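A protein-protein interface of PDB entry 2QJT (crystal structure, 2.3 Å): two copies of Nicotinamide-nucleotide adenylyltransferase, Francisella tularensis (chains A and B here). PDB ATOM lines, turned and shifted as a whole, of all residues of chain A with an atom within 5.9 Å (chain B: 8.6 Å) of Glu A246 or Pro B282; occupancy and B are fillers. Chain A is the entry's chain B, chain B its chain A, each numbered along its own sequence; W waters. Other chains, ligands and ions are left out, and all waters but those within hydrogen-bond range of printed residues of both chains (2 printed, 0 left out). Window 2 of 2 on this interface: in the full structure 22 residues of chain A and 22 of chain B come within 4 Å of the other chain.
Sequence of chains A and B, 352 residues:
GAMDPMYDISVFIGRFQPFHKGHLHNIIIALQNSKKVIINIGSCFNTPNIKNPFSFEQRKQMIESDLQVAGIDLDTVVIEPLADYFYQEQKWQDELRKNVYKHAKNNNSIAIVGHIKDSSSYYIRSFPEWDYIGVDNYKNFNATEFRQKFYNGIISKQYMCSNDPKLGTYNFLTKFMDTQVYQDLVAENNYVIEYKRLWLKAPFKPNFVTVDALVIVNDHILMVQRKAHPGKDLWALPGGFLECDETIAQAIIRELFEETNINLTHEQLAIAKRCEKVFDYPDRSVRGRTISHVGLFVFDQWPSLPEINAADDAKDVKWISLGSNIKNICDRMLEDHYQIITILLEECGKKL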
ATOM      1  N   PHE A 241     -15.223  26.749  24.831  1.00  0.00           N
ATOM      2  CA  PHE A 241     -15.390  25.940  23.647  1.00  0.00           C
ATOM      3  C   PHE A 241     -15.980  26.755  22.524  1.00  0.00           C
ATOM      4  O   PHE A 241     -16.847  27.617  22.722  1.00  0.00           O
ATOM      5  CB  PHE A 241     -16.215  24.675  23.973  1.00  0.00           C
ATOM      6  CG  PHE A 241     -15.419  23.612  24.719  1.00  0.00           C
ATOM      7  CD1 PHE A 241     -15.429  23.559  26.108  1.00  0.00           C
ATOM      8  CD2 PHE A 241     -14.617  22.686  24.020  1.00  0.00           C
ATOM      9  CE1 PHE A 241     -14.653  22.579  26.808  1.00  0.00           C
ATOM     10  CE2 PHE A 241     -13.841  21.707  24.709  1.00  0.00           C
ATOM     11  CZ  PHE A 241     -13.861  21.666  26.099  1.00  0.00           C
ATOM     12  N   LEU A 242     -15.473  26.500  21.335  1.00  0.00           N
ATOM     13  CA  LEU A 242     -16.033  27.019  20.105  1.00  0.00           C
ATOM     14  C   LEU A 242     -17.278  26.212  19.751  1.00  0.00           C
ATOM     15  O   LEU A 242     -17.260  24.961  19.767  1.00  0.00           O
ATOM     16  CB  LEU A 242     -14.982  26.891  18.993  1.00  0.00           C
ATOM     17  CG  LEU A 242     -15.454  27.092  17.558  1.00  0.00           C
ATOM     18  CD1 LEU A 242     -15.803  28.563  17.342  1.00  0.00           C
ATOM     19  CD2 LEU A 242     -14.386  26.619  16.586  1.00  0.00           C
ATOM     20  N   GLU A 243     -18.357  26.922  19.439  1.00  0.00           N
ATOM     21  CA  GLU A 243     -19.630  26.289  19.076  1.00  0.00           C
ATOM     22  C   GLU A 243     -19.673  26.154  17.579  1.00  0.00           C
ATOM     23  O   GLU A 243     -18.874  26.771  16.877  1.00  0.00           O
ATOM     24  CB  GLU A 243     -20.838  27.098  19.602  1.00  0.00           C
ATOM     25  CG  GLU A 243     -20.740  27.476  21.066  1.00  0.00           C
ATOM     26  CD  GLU A 243     -20.979  26.320  22.031  1.00  0.00           C
ATOM     27  OE1 GLU A 243     -20.506  26.376  23.197  1.00  0.00           O
ATOM     28  OE2 GLU A 243     -21.639  25.341  21.633  1.00  0.00           O
ATOM     29  N   CYS A 244     -20.610  25.356  17.098  1.00  0.00           N
ATOM     30  CA  CYS A 244     -20.635  24.916  15.720  1.00  0.00           C
ATOM     31  C   CYS A 244     -21.172  25.954  14.751  1.00  0.00           C
ATOM     32  O   CYS A 244     -20.964  25.870  13.530  1.00  0.00           O
ATOM     33  CB  CYS A 244     -21.447  23.616  15.613  1.00  0.00           C
ATOM     34  SG  CYS A 244     -20.408  22.215  16.187  1.00  0.00           S
ATOM     35  N   ASP A 245     -21.898  26.925  15.285  1.00  0.00           N
ATOM     36  CA  ASP A 245     -22.578  27.860  14.408  1.00  0.00           C
ATOM     37  C   ASP A 245     -21.910  29.229  14.399  1.00  0.00           C
ATOM     38  O   ASP A 245     -22.410  30.150  13.789  1.00  0.00           O
ATOM     39  CB  ASP A 245     -24.075  27.931  14.749  1.00  0.00           C
ATOM     40  CG  ASP A 245     -24.343  28.263  16.233  1.00  0.00           C
ATOM     41  OD1 ASP A 245     -25.545  28.273  16.611  1.00  0.00           O
ATOM     42  OD2 ASP A 245     -23.384  28.490  17.023  1.00  0.00           O
ATOM     43  N   GLU A 246     -20.747  29.337  15.022  1.00  0.00           N
ATOM     44  CA  GLU A 246     -20.019  30.616  15.089  1.00  0.00           C
ATOM     45  C   GLU A 246     -18.607  30.519  14.540  1.00  0.00           C
ATOM     46  O   GLU A 246     -17.922  29.484  14.684  1.00  0.00           O
ATOM     47  CB  GLU A 246     -19.958  31.129  16.526  1.00  0.00           C
ATOM     48  CG  GLU A 246     -19.218  30.166  17.427  1.00  0.00           C
ATOM     49  CD  GLU A 246     -19.234  30.555  18.884  1.00  0.00           C
ATOM     50  OE1 GLU A 246     -18.638  29.831  19.726  1.00  0.00           O
ATOM     51  OE2 GLU A 246     -19.827  31.589  19.192  1.00  0.00           O
ATOM     52  N   THR A 247     -18.139  31.614  13.949  1.00  0.00           N
ATOM     53  CA  THR A 247     -16.714  31.728  13.654  1.00  0.00           C
ATOM     54  C   THR A 247     -15.887  31.799  14.946  1.00  0.00           C
ATOM     55  O   THR A 247     -16.419  32.003  16.035  1.00  0.00           O
ATOM     56  CB  THR A 247     -16.381  32.980  12.815  1.00  0.00           C
ATOM     57  OG1 THR A 247     -16.593  34.109  13.646  1.00  0.00           O
ATOM     58  CG2 THR A 247     -17.244  33.063  11.601  1.00  0.00           C
ATOM     59  N   ILE A 248     -14.579  31.636  14.790  1.00  0.00           N
ATOM     60  CA  ILE A 248     -13.611  31.758  15.872  1.00  0.00           C
ATOM     61  C   ILE A 248     -13.520  33.170  16.424  1.00  0.00           C
ATOM     62  O   ILE A 248     -13.414  33.340  17.642  1.00  0.00           O
ATOM     63  CB  ILE A 248     -12.202  31.258  15.403  1.00  0.00           C
ATOM     64  CG1 ILE A 248     -12.199  29.726  15.377  1.00  0.00           C
ATOM     65  CG2 ILE A 248     -11.105  31.759  16.345  1.00  0.00           C
ATOM     66  CD1 ILE A 248     -11.284  29.143  14.409  1.00  0.00           C
ATOM     67  N   GLN A 250     -15.947  35.357  16.445  1.00  0.00           N
ATOM     68  CA  GLN A 250     -17.179  35.543  17.238  1.00  0.00           C
ATOM     69  C   GLN A 250     -17.126  34.845  18.585  1.00  0.00           C
ATOM     70  O   GLN A 250     -17.548  35.420  19.607  1.00  0.00           O
ATOM     71  CB  GLN A 250     -18.414  35.063  16.453  1.00  0.00           C
ATOM     72  CG  GLN A 250     -18.697  35.879  15.174  1.00  0.00           C
ATOM     73  CD  GLN A 250     -19.717  35.213  14.257  1.00  0.00           C
ATOM     74  OE1 GLN A 250     -19.856  33.980  14.216  1.00  0.00           O
ATOM     75  NE2 GLN A 250     -20.431  36.035  13.483  1.00  0.00           N
ATOM     76  N   ALA A 251     -16.603  33.603  18.575  1.00  0.00           N
ATOM     77  CA  ALA A 251     -16.436  32.784  19.764  1.00  0.00           C
ATOM     78  C   ALA A 251     -15.574  33.467  20.785  1.00  0.00           C
ATOM     79  O   ALA A 251     -15.896  33.430  21.977  1.00  0.00           O
ATOM     80  CB  ALA A 251     -15.823  31.402  19.393  1.00  0.00           C
ATOM     81  N   ARG A 254     -17.718  36.236  22.214  1.00  0.00           N
ATOM     82  CA  ARG A 254     -18.828  35.658  23.004  1.00  0.00           C
ATOM     83  C   ARG A 254     -18.399  35.164  24.415  1.00  0.00           C
ATOM     84  O   ARG A 254     -19.048  35.509  25.411  1.00  0.00           O
ATOM     85  CB  ARG A 254     -19.586  34.577  22.220  1.00  0.00           C
ATOM     86  CG  ARG A 254     -20.601  33.802  23.075  1.00  0.00           C
ATOM     87  CD  ARG A 254     -21.231  32.568  22.353  1.00  0.00           C
ATOM     88  NE  ARG A 254     -20.192  31.622  21.909  1.00  0.00           N
ATOM     89  CZ  ARG A 254     -19.486  30.837  22.722  1.00  0.00           C
ATOM     90  NH1 ARG A 254     -18.543  30.060  22.217  1.00  0.00           N
ATOM     91  NH2 ARG A 254     -19.707  30.848  24.030  1.00  0.00           N
ATOM     92  N   PHE B  86     -16.661  33.887   1.721  1.00  0.00           N
ATOM     93  CA  PHE B  86     -16.899  33.684   3.153  1.00  0.00           C
ATOM     94  C   PHE B  86     -15.897  34.427   4.057  1.00  0.00           C
ATOM     95  O   PHE B  86     -16.174  34.645   5.227  1.00  0.00           O
ATOM     96  CB  PHE B  86     -16.807  32.189   3.533  1.00  0.00           C
ATOM     97  CG  PHE B  86     -17.633  31.257   2.697  1.00  0.00           C
ATOM     98  CD1 PHE B  86     -17.120  29.993   2.388  1.00  0.00           C
ATOM     99  CD2 PHE B  86     -18.910  31.606   2.238  1.00  0.00           C
ATOM    100  CE1 PHE B  86     -17.858  29.082   1.642  1.00  0.00           C
ATOM    101  CE2 PHE B  86     -19.660  30.727   1.488  1.00  0.00           C
ATOM    102  CZ  PHE B  86     -19.146  29.456   1.164  1.00  0.00           C
ATOM    103  N   TYR B  87     -14.714  34.759   3.537  1.00  0.00           N
ATOM    104  CA  TYR B  87     -13.648  35.327   4.353  1.00  0.00           C
ATOM    105  C   TYR B  87     -13.280  36.753   3.908  1.00  0.00           C
ATOM    106  O   TYR B  87     -12.375  37.352   4.477  1.00  0.00           O
ATOM    107  CB  TYR B  87     -12.385  34.407   4.321  1.00  0.00           C
ATOM    108  CG  TYR B  87     -12.721  32.936   4.501  1.00  0.00           C
ATOM    109  CD1 TYR B  87     -12.836  32.068   3.387  1.00  0.00           C
ATOM    110  CD2 TYR B  87     -12.991  32.435   5.776  1.00  0.00           C
ATOM    111  CE1 TYR B  87     -13.182  30.771   3.563  1.00  0.00           C
ATOM    112  CE2 TYR B  87     -13.356  31.151   5.956  1.00  0.00           C
ATOM    113  CZ  TYR B  87     -13.444  30.313   4.868  1.00  0.00           C
ATOM    114  OH  TYR B  87     -13.816  29.016   5.108  1.00  0.00           O
ATOM    115  N   LYS B 205     -21.666  18.043  19.941  1.00  0.00           N
ATOM    116  CA  LYS B 205     -21.563  18.210  18.480  1.00  0.00           C
ATOM    117  C   LYS B 205     -20.109  18.577  18.022  1.00  0.00           C
ATOM    118  O   LYS B 205     -19.513  19.556  18.499  1.00  0.00           O
ATOM    119  CB  LYS B 205     -22.592  19.261  18.019  1.00  0.00           C
ATOM    120  CG  LYS B 205     -23.176  19.046  16.619  1.00  0.00           C
ATOM    121  CD  LYS B 205     -24.001  20.261  16.205  1.00  0.00           C
ATOM    122  CE  LYS B 205     -24.014  20.436  14.677  1.00  0.00           C
ATOM    123  NZ  LYS B 205     -25.096  21.397  14.223  1.00  0.00           N
ATOM    124  N   PRO B 206     -19.530  17.777  17.106  1.00  0.00           N
ATOM    125  CA  PRO B 206     -18.066  17.900  16.919  1.00  0.00           C
ATOM    126  C   PRO B 206     -17.618  19.015  15.941  1.00  0.00           C
ATOM    127  O   PRO B 206     -18.310  19.325  14.963  1.00  0.00           O
ATOM    128  CB  PRO B 206     -17.657  16.509  16.431  1.00  0.00           C
ATOM    129  CG  PRO B 206     -19.015  15.771  16.110  1.00  0.00           C
ATOM    130  CD  PRO B 206     -20.114  16.769  16.206  1.00  0.00           C
ATOM    131  N   ASN B 207     -16.527  19.686  16.283  1.00  0.00           N
ATOM    132  CA  ASN B 207     -15.776  20.481  15.313  1.00  0.00           C
ATOM    133  C   ASN B 207     -14.699  19.543  14.738  1.00  0.00           C
ATOM    134  O   ASN B 207     -13.963  18.905  15.485  1.00  0.00           O
ATOM    135  CB  ASN B 207     -15.105  21.684  15.973  1.00  0.00           C
ATOM    136  CG  ASN B 207     -16.086  22.745  16.453  1.00  0.00           C
ATOM    137  OD1 ASN B 207     -16.924  23.239  15.712  1.00  0.00           O
ATOM    138  ND2 ASN B 207     -15.943  23.132  17.698  1.00  0.00           N
ATOM    139  N   PHE B 279      -9.332  28.463   8.292  1.00  0.00           N
ATOM    140  CA  PHE B 279     -10.553  28.671   7.557  1.00  0.00           C
ATOM    141  C   PHE B 279     -11.691  28.009   8.310  1.00  0.00           C
ATOM    142  O   PHE B 279     -11.688  26.789   8.525  1.00  0.00           O
ATOM    143  CB  PHE B 279     -10.373  28.249   6.093  1.00  0.00           C
ATOM    144  CG  PHE B 279      -9.296  29.077   5.367  1.00  0.00           C
ATOM    145  CD1 PHE B 279      -7.970  28.653   5.337  1.00  0.00           C
ATOM    146  CD2 PHE B 279      -9.622  30.320   4.776  1.00  0.00           C
ATOM    147  CE1 PHE B 279      -6.967  29.440   4.700  1.00  0.00           C
ATOM    148  CE2 PHE B 279      -8.647  31.121   4.112  1.00  0.00           C
ATOM    149  CZ  PHE B 279      -7.321  30.685   4.081  1.00  0.00           C
ATOM    150  N   ASP B 280     -12.643  28.834   8.751  1.00  0.00           N
ATOM    151  CA  ASP B 280     -13.602  28.450   9.798  1.00  0.00           C
ATOM    152  C   ASP B 280     -15.037  28.868   9.499  1.00  0.00           C
ATOM    153  O   ASP B 280     -15.832  28.972  10.447  1.00  0.00           O
ATOM    154  CB  ASP B 280     -13.221  29.084  11.156  1.00  0.00           C
ATOM    155  CG  ASP B 280     -13.239  30.619  11.107  1.00  0.00           C
ATOM    156  OD1 ASP B 280     -13.106  31.143  10.002  1.00  0.00           O
ATOM    157  OD2 ASP B 280     -13.415  31.298  12.143  1.00  0.00           O
ATOM    158  N   TYR B 281     -15.364  29.148   8.232  1.00  0.00           N
ATOM    159  CA  TYR B 281     -16.759  29.387   7.847  1.00  0.00           C
ATOM    160  C   TYR B 281     -17.596  28.137   8.264  1.00  0.00           C
ATOM    161  O   TYR B 281     -17.249  27.039   7.876  1.00  0.00           O
ATOM    162  CB  TYR B 281     -16.880  29.662   6.332  1.00  0.00           C
ATOM    163  CG  TYR B 281     -18.307  29.859   5.864  1.00  0.00           C
ATOM    164  CD1 TYR B 281     -19.032  31.019   6.210  1.00  0.00           C
ATOM    165  CD2 TYR B 281     -18.939  28.891   5.073  1.00  0.00           C
ATOM    166  CE1 TYR B 281     -20.349  31.208   5.775  1.00  0.00           C
ATOM    167  CE2 TYR B 281     -20.258  29.051   4.643  1.00  0.00           C
ATOM    168  CZ  TYR B 281     -20.959  30.215   4.998  1.00  0.00           C
ATOM    169  OH  TYR B 281     -22.249  30.369   4.559  1.00  0.00           O
ATOM    170  N   PRO B 282     -18.620  28.298   9.141  1.00  0.00           N
ATOM    171  CA  PRO B 282     -19.299  27.118   9.738  1.00  0.00           C
ATOM    172  C   PRO B 282     -19.858  26.095   8.763  1.00  0.00           C
ATOM    173  O   PRO B 282     -19.780  24.901   9.050  1.00  0.00           O
ATOM    174  CB  PRO B 282     -20.350  27.749  10.628  1.00  0.00           C
ATOM    175  CG  PRO B 282     -19.663  29.089  11.038  1.00  0.00           C
ATOM    176  CD  PRO B 282     -19.112  29.556   9.735  1.00  0.00           C
ATOM    177  N   ASP B 283     -20.288  26.524   7.575  1.00  0.00           N
ATOM    178  CA  ASP B 283     -20.833  25.612   6.579  1.00  0.00           C
ATOM    179  C   ASP B 283     -19.985  25.329   5.378  1.00  0.00           C
ATOM    180  O   ASP B 283     -20.524  24.878   4.364  1.00  0.00           O
ATOM    181  CB  ASP B 283     -22.180  26.132   6.059  1.00  0.00           C
ATOM    182  CG  ASP B 283     -23.052  26.585   7.168  1.00  0.00           C
ATOM    183  OD1 ASP B 283     -23.227  25.797   8.121  1.00  0.00           O
ATOM    184  OD2 ASP B 283     -23.523  27.745   7.115  1.00  0.00           O
ATOM    185  N   ARG B 284     -18.679  25.600   5.469  1.00  0.00           N
ATOM    186  CA  ARG B 284     -17.734  25.292   4.380  1.00  0.00           C
ATOM    187  C   ARG B 284     -17.785  23.826   3.921  1.00  0.00           C
ATOM    188  O   ARG B 284     -17.631  23.546   2.735  1.00  0.00           O
ATOM    189  CB  ARG B 284     -16.292  25.716   4.737  1.00  0.00           C
ATOM    190  CG  ARG B 284     -15.724  25.166   6.043  1.00  0.00           C
ATOM    191  CD  ARG B 284     -14.370  25.787   6.397  1.00  0.00           C
ATOM    192  NE  ARG B 284     -13.467  25.570   5.302  1.00  0.00           N
ATOM    193  CZ  ARG B 284     -12.701  24.486   5.164  1.00  0.00           C
ATOM    194  NH1 ARG B 284     -12.711  23.539   6.108  1.00  0.00           N
ATOM    195  NH2 ARG B 284     -11.925  24.342   4.081  1.00  0.00           N
ATOM    196  N   SER B 285     -18.033  22.892   4.827  1.00  0.00           N
ATOM    197  CA  SER B 285     -18.079  21.482   4.453  1.00  0.00           C
ATOM    198  C   SER B 285     -19.399  20.782   4.849  1.00  0.00           C
ATOM    199  O   SER B 285     -19.951  21.066   5.919  1.00  0.00           O
ATOM    200  CB  SER B 285     -16.883  20.753   5.085  1.00  0.00           C
ATOM    201  OG  SER B 285     -16.986  19.353   4.914  1.00  0.00           O
ATOM    202  N   VAL B 286     -19.856  19.837   4.010  1.00  0.00           N
ATOM    203  CA  VAL B 286     -21.127  19.059   4.246  1.00  0.00           C
ATOM    204  C   VAL B 286     -21.128  17.945   5.334  1.00  0.00           C
ATOM    205  O   VAL B 286     -22.204  17.516   5.771  1.00  0.00           O
ATOM    206  CB  VAL B 286     -21.717  18.440   2.934  1.00  0.00           C
ATOM    207  CG1 VAL B 286     -22.123  19.519   1.904  1.00  0.00           C
ATOM    208  CG2 VAL B 286     -20.757  17.418   2.317  1.00  0.00           C
ATOM    209  N   ARG B 287     -19.945  17.496   5.773  1.00  0.00           N
ATOM    210  CA  ARG B 287     -19.792  16.468   6.826  1.00  0.00           C
ATOM    211  C   ARG B 287     -20.245  16.942   8.200  1.00  0.00           C
ATOM    212  O   ARG B 287     -20.583  16.153   9.072  1.00  0.00           O
ATOM    213  CB  ARG B 287     -18.321  16.085   6.969  1.00  0.00           C
ATOM    214  CG  ARG B 287     -17.877  14.775   6.316  1.00  0.00           C
ATOM    215  CD  ARG B 287     -16.429  14.479   6.779  1.00  0.00           C
ATOM    216  NE  ARG B 287     -15.739  15.756   6.869  1.00  0.00           N
ATOM    217  CZ  ARG B 287     -14.795  16.179   6.019  1.00  0.00           C
ATOM    218  NH1 ARG B 287     -14.326  15.387   5.049  1.00  0.00           N
ATOM    219  NH2 ARG B 287     -14.310  17.410   6.174  1.00  0.00           N
ATOM    220  N   GLY B 288     -20.197  18.247   8.410  1.00  0.00           N
ATOM    221  CA  GLY B 288     -20.239  18.797   9.753  1.00  0.00           C
ATOM    222  C   GLY B 288     -19.256  19.944   9.786  1.00  0.00           C
ATOM    223  O   GLY B 288     -18.656  20.272   8.757  1.00  0.00           O
ATOM    224  N   ARG B 289     -19.065  20.533  10.968  1.00  0.00           N
ATOM    225  CA  ARG B 289     -18.263  21.716  11.080  1.00  0.00           C
ATOM    226  C   ARG B 289     -16.785  21.374  11.083  1.00  0.00           C
ATOM    227  O   ARG B 289     -16.280  20.759  12.008  1.00  0.00           O
ATOM    228  CB  ARG B 289     -18.635  22.555  12.294  1.00  0.00           C
ATOM    229  CG  ARG B 289     -18.299  24.008  12.110  1.00  0.00           C
ATOM    230  CD  ARG B 289     -16.881  24.336  12.610  1.00  0.00           C
ATOM    231  NE  ARG B 289     -16.570  25.742  12.371  1.00  0.00           N
ATOM    232  CZ  ARG B 289     -16.838  26.704  13.241  1.00  0.00           C
ATOM    233  NH1 ARG B 289     -17.410  26.395  14.395  1.00  0.00           N
ATOM    234  NH2 ARG B 289     -16.556  27.977  12.957  1.00  0.00           N
ATOM    235  N   THR B 290     -16.112  21.835  10.028  1.00  0.00           N
ATOM    236  CA  THR B 290     -14.709  21.508   9.715  1.00  0.00           C
ATOM    237  C   THR B 290     -13.915  22.818   9.572  1.00  0.00           C
ATOM    238  O   THR B 290     -14.239  23.667   8.750  1.00  0.00           O
ATOM    239  CB  THR B 290     -14.659  20.679   8.418  1.00  0.00           C
ATOM    240  OG1 THR B 290     -15.546  19.569   8.576  1.00  0.00           O
ATOM    241  CG2 THR B 290     -13.245  20.181   8.093  1.00  0.00           C
ATOM    242  N   ILE B 291     -12.936  22.973  10.446  1.00  0.00           N
ATOM    243  CA  ILE B 291     -11.991  24.070  10.448  1.00  0.00           C
ATOM    244  C   ILE B 291     -10.721  23.557   9.825  1.00  0.00           C
ATOM    245  O   ILE B 291     -10.176  22.504  10.236  1.00  0.00           O
ATOM    246  CB  ILE B 291     -11.678  24.526  11.872  1.00  0.00           C
ATOM    247  CG1 ILE B 291     -12.968  24.957  12.570  1.00  0.00           C
ATOM    248  CG2 ILE B 291     -10.654  25.717  11.870  1.00  0.00           C
ATOM    249  CD1 ILE B 291     -12.872  24.983  14.030  1.00  0.00           C
ATOM    250  N   ASP B 336     -14.563  25.369  -0.204  1.00  0.00           N
ATOM    251  CA  ASP B 336     -14.039  26.732  -0.342  1.00  0.00           C
ATOM    252  C   ASP B 336     -12.581  26.840  -0.824  1.00  0.00           C
ATOM    253  O   ASP B 336     -11.940  27.869  -0.583  1.00  0.00           O
ATOM    254  CB  ASP B 336     -14.173  27.472   1.005  1.00  0.00           C
ATOM    255  CG  ASP B 336     -13.483  26.726   2.164  1.00  0.00           C
ATOM    256  OD1 ASP B 336     -13.415  27.258   3.308  1.00  0.00           O
ATOM    257  OD2 ASP B 336     -13.044  25.582   1.943  1.00  0.00           O
HETATM  258  O   HOH W   1     -15.127  22.436  20.491  1.00  0.00           O
HETATM  259  O   HOH W   2     -20.517  19.532  13.622  1.00  0.00           O
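The side-chain carboxylate of Glu A246 is in hydrogen-bond range of the backbone NH of Glu A243 (2.9 Å). The side-chain carboxylate (OE1) of Glu A246 lies within salt-bridge range of the guanidinium group (NH1) of Arg A254, 2.5 Å away. The side-chain amide oxygen (OE1) of Gln A250 is in hydrogen-bond range of the backbone NH (N) of Thr A247 (2.9 Å). OD1 of Asn B207 sits close to NH1 of Arg B289. O of Asp B280 sits at hydrogen-bond distance from NH2 of Arg B289 (2.8 Å).
Pro B282 touches two residues of chain A. Thr A247 touches two residues of chain B. Of the printed residues of chain B, Glu A243 touches Arg B289. Of the printed residues of chain B, Cys A244 touches Lys B205, Pro B206, Asn B207, Pro B282 and Arg B289. Of the printed residues of chain A, Lys B205 touches Cys A244 (3.6 Å). Of the printed residues of chain B, Ile A248 touches Asp B280. Of the printed residues of chain A, Pro B206 touches Cys A244. The nearest residue of chain B that does not touch Glu A246 is Asp B280 (4.8 Å).
Water W2 lies within hydrogen-bond range of O of Pro B206 (2.6 Å), N of Arg B289 (3.2 Å) and SG of Cys A244 (3.7 Å). Water W1 bridges ND2 of Asn B207 and O of Leu A242.
O of Leu A242 sits at hydrogen-bond distance from ND2 of Asn B207. O of Glu A243 is in hydrogen-bond range of NH1 of Arg B289, 2.9 Å away. O of Lys B205 lies within hydrogen-bond range of SG of Cys A244, 3.6 Å away. The side-chain sulfur of Cys A244 sits at hydrogen-bond distance from the backbone carbonyl oxygen of Pro B206 (3.8 Å). SG of Cys A244 sits at hydrogen-bond distance from OD1 of Asn B207, 3.7 Å away. The backbone carbonyl oxygen (O) of Glu A246 is in hydrogen-bond range of the guanidinium group (NH2) of Arg B289 (2.7 Å). OD2 of Asp B280 sits at hydrogen-bond distance from N of Ile A248, at 2.9 Å.
Printed residues of chain A that touch a printed residue of chain B: Leu A242, Glu A243, Cys A244, Glu A246, Thr A247 and Ile A248. Hydrophobic or aromatic side chains of chain A that line the printed part of chain B: Leu A242 and Ile A248. Hydrophobic or aromatic side chains of chain B that line the printed part of chain A: Pro B282 and Ile B291. Among the printed residues, 14 pairs touch across the chains.
Among the printed residues, pairs that only touch across the chains: Leu A242 with Ile B291 (3.4 Å), Thr A247 with Asp B280 (3.5 Å), Cys A244 with Pro B282 (3.5 Å), Cys A244 with Arg B289 (3.5 Å), Leu A242 with Arg B289 (3.7 Å), Thr A247 with Arg B289 (3.8 Å) and Glu A246 with Pro B282 (3.9 Å).
No position is printed for both chains.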
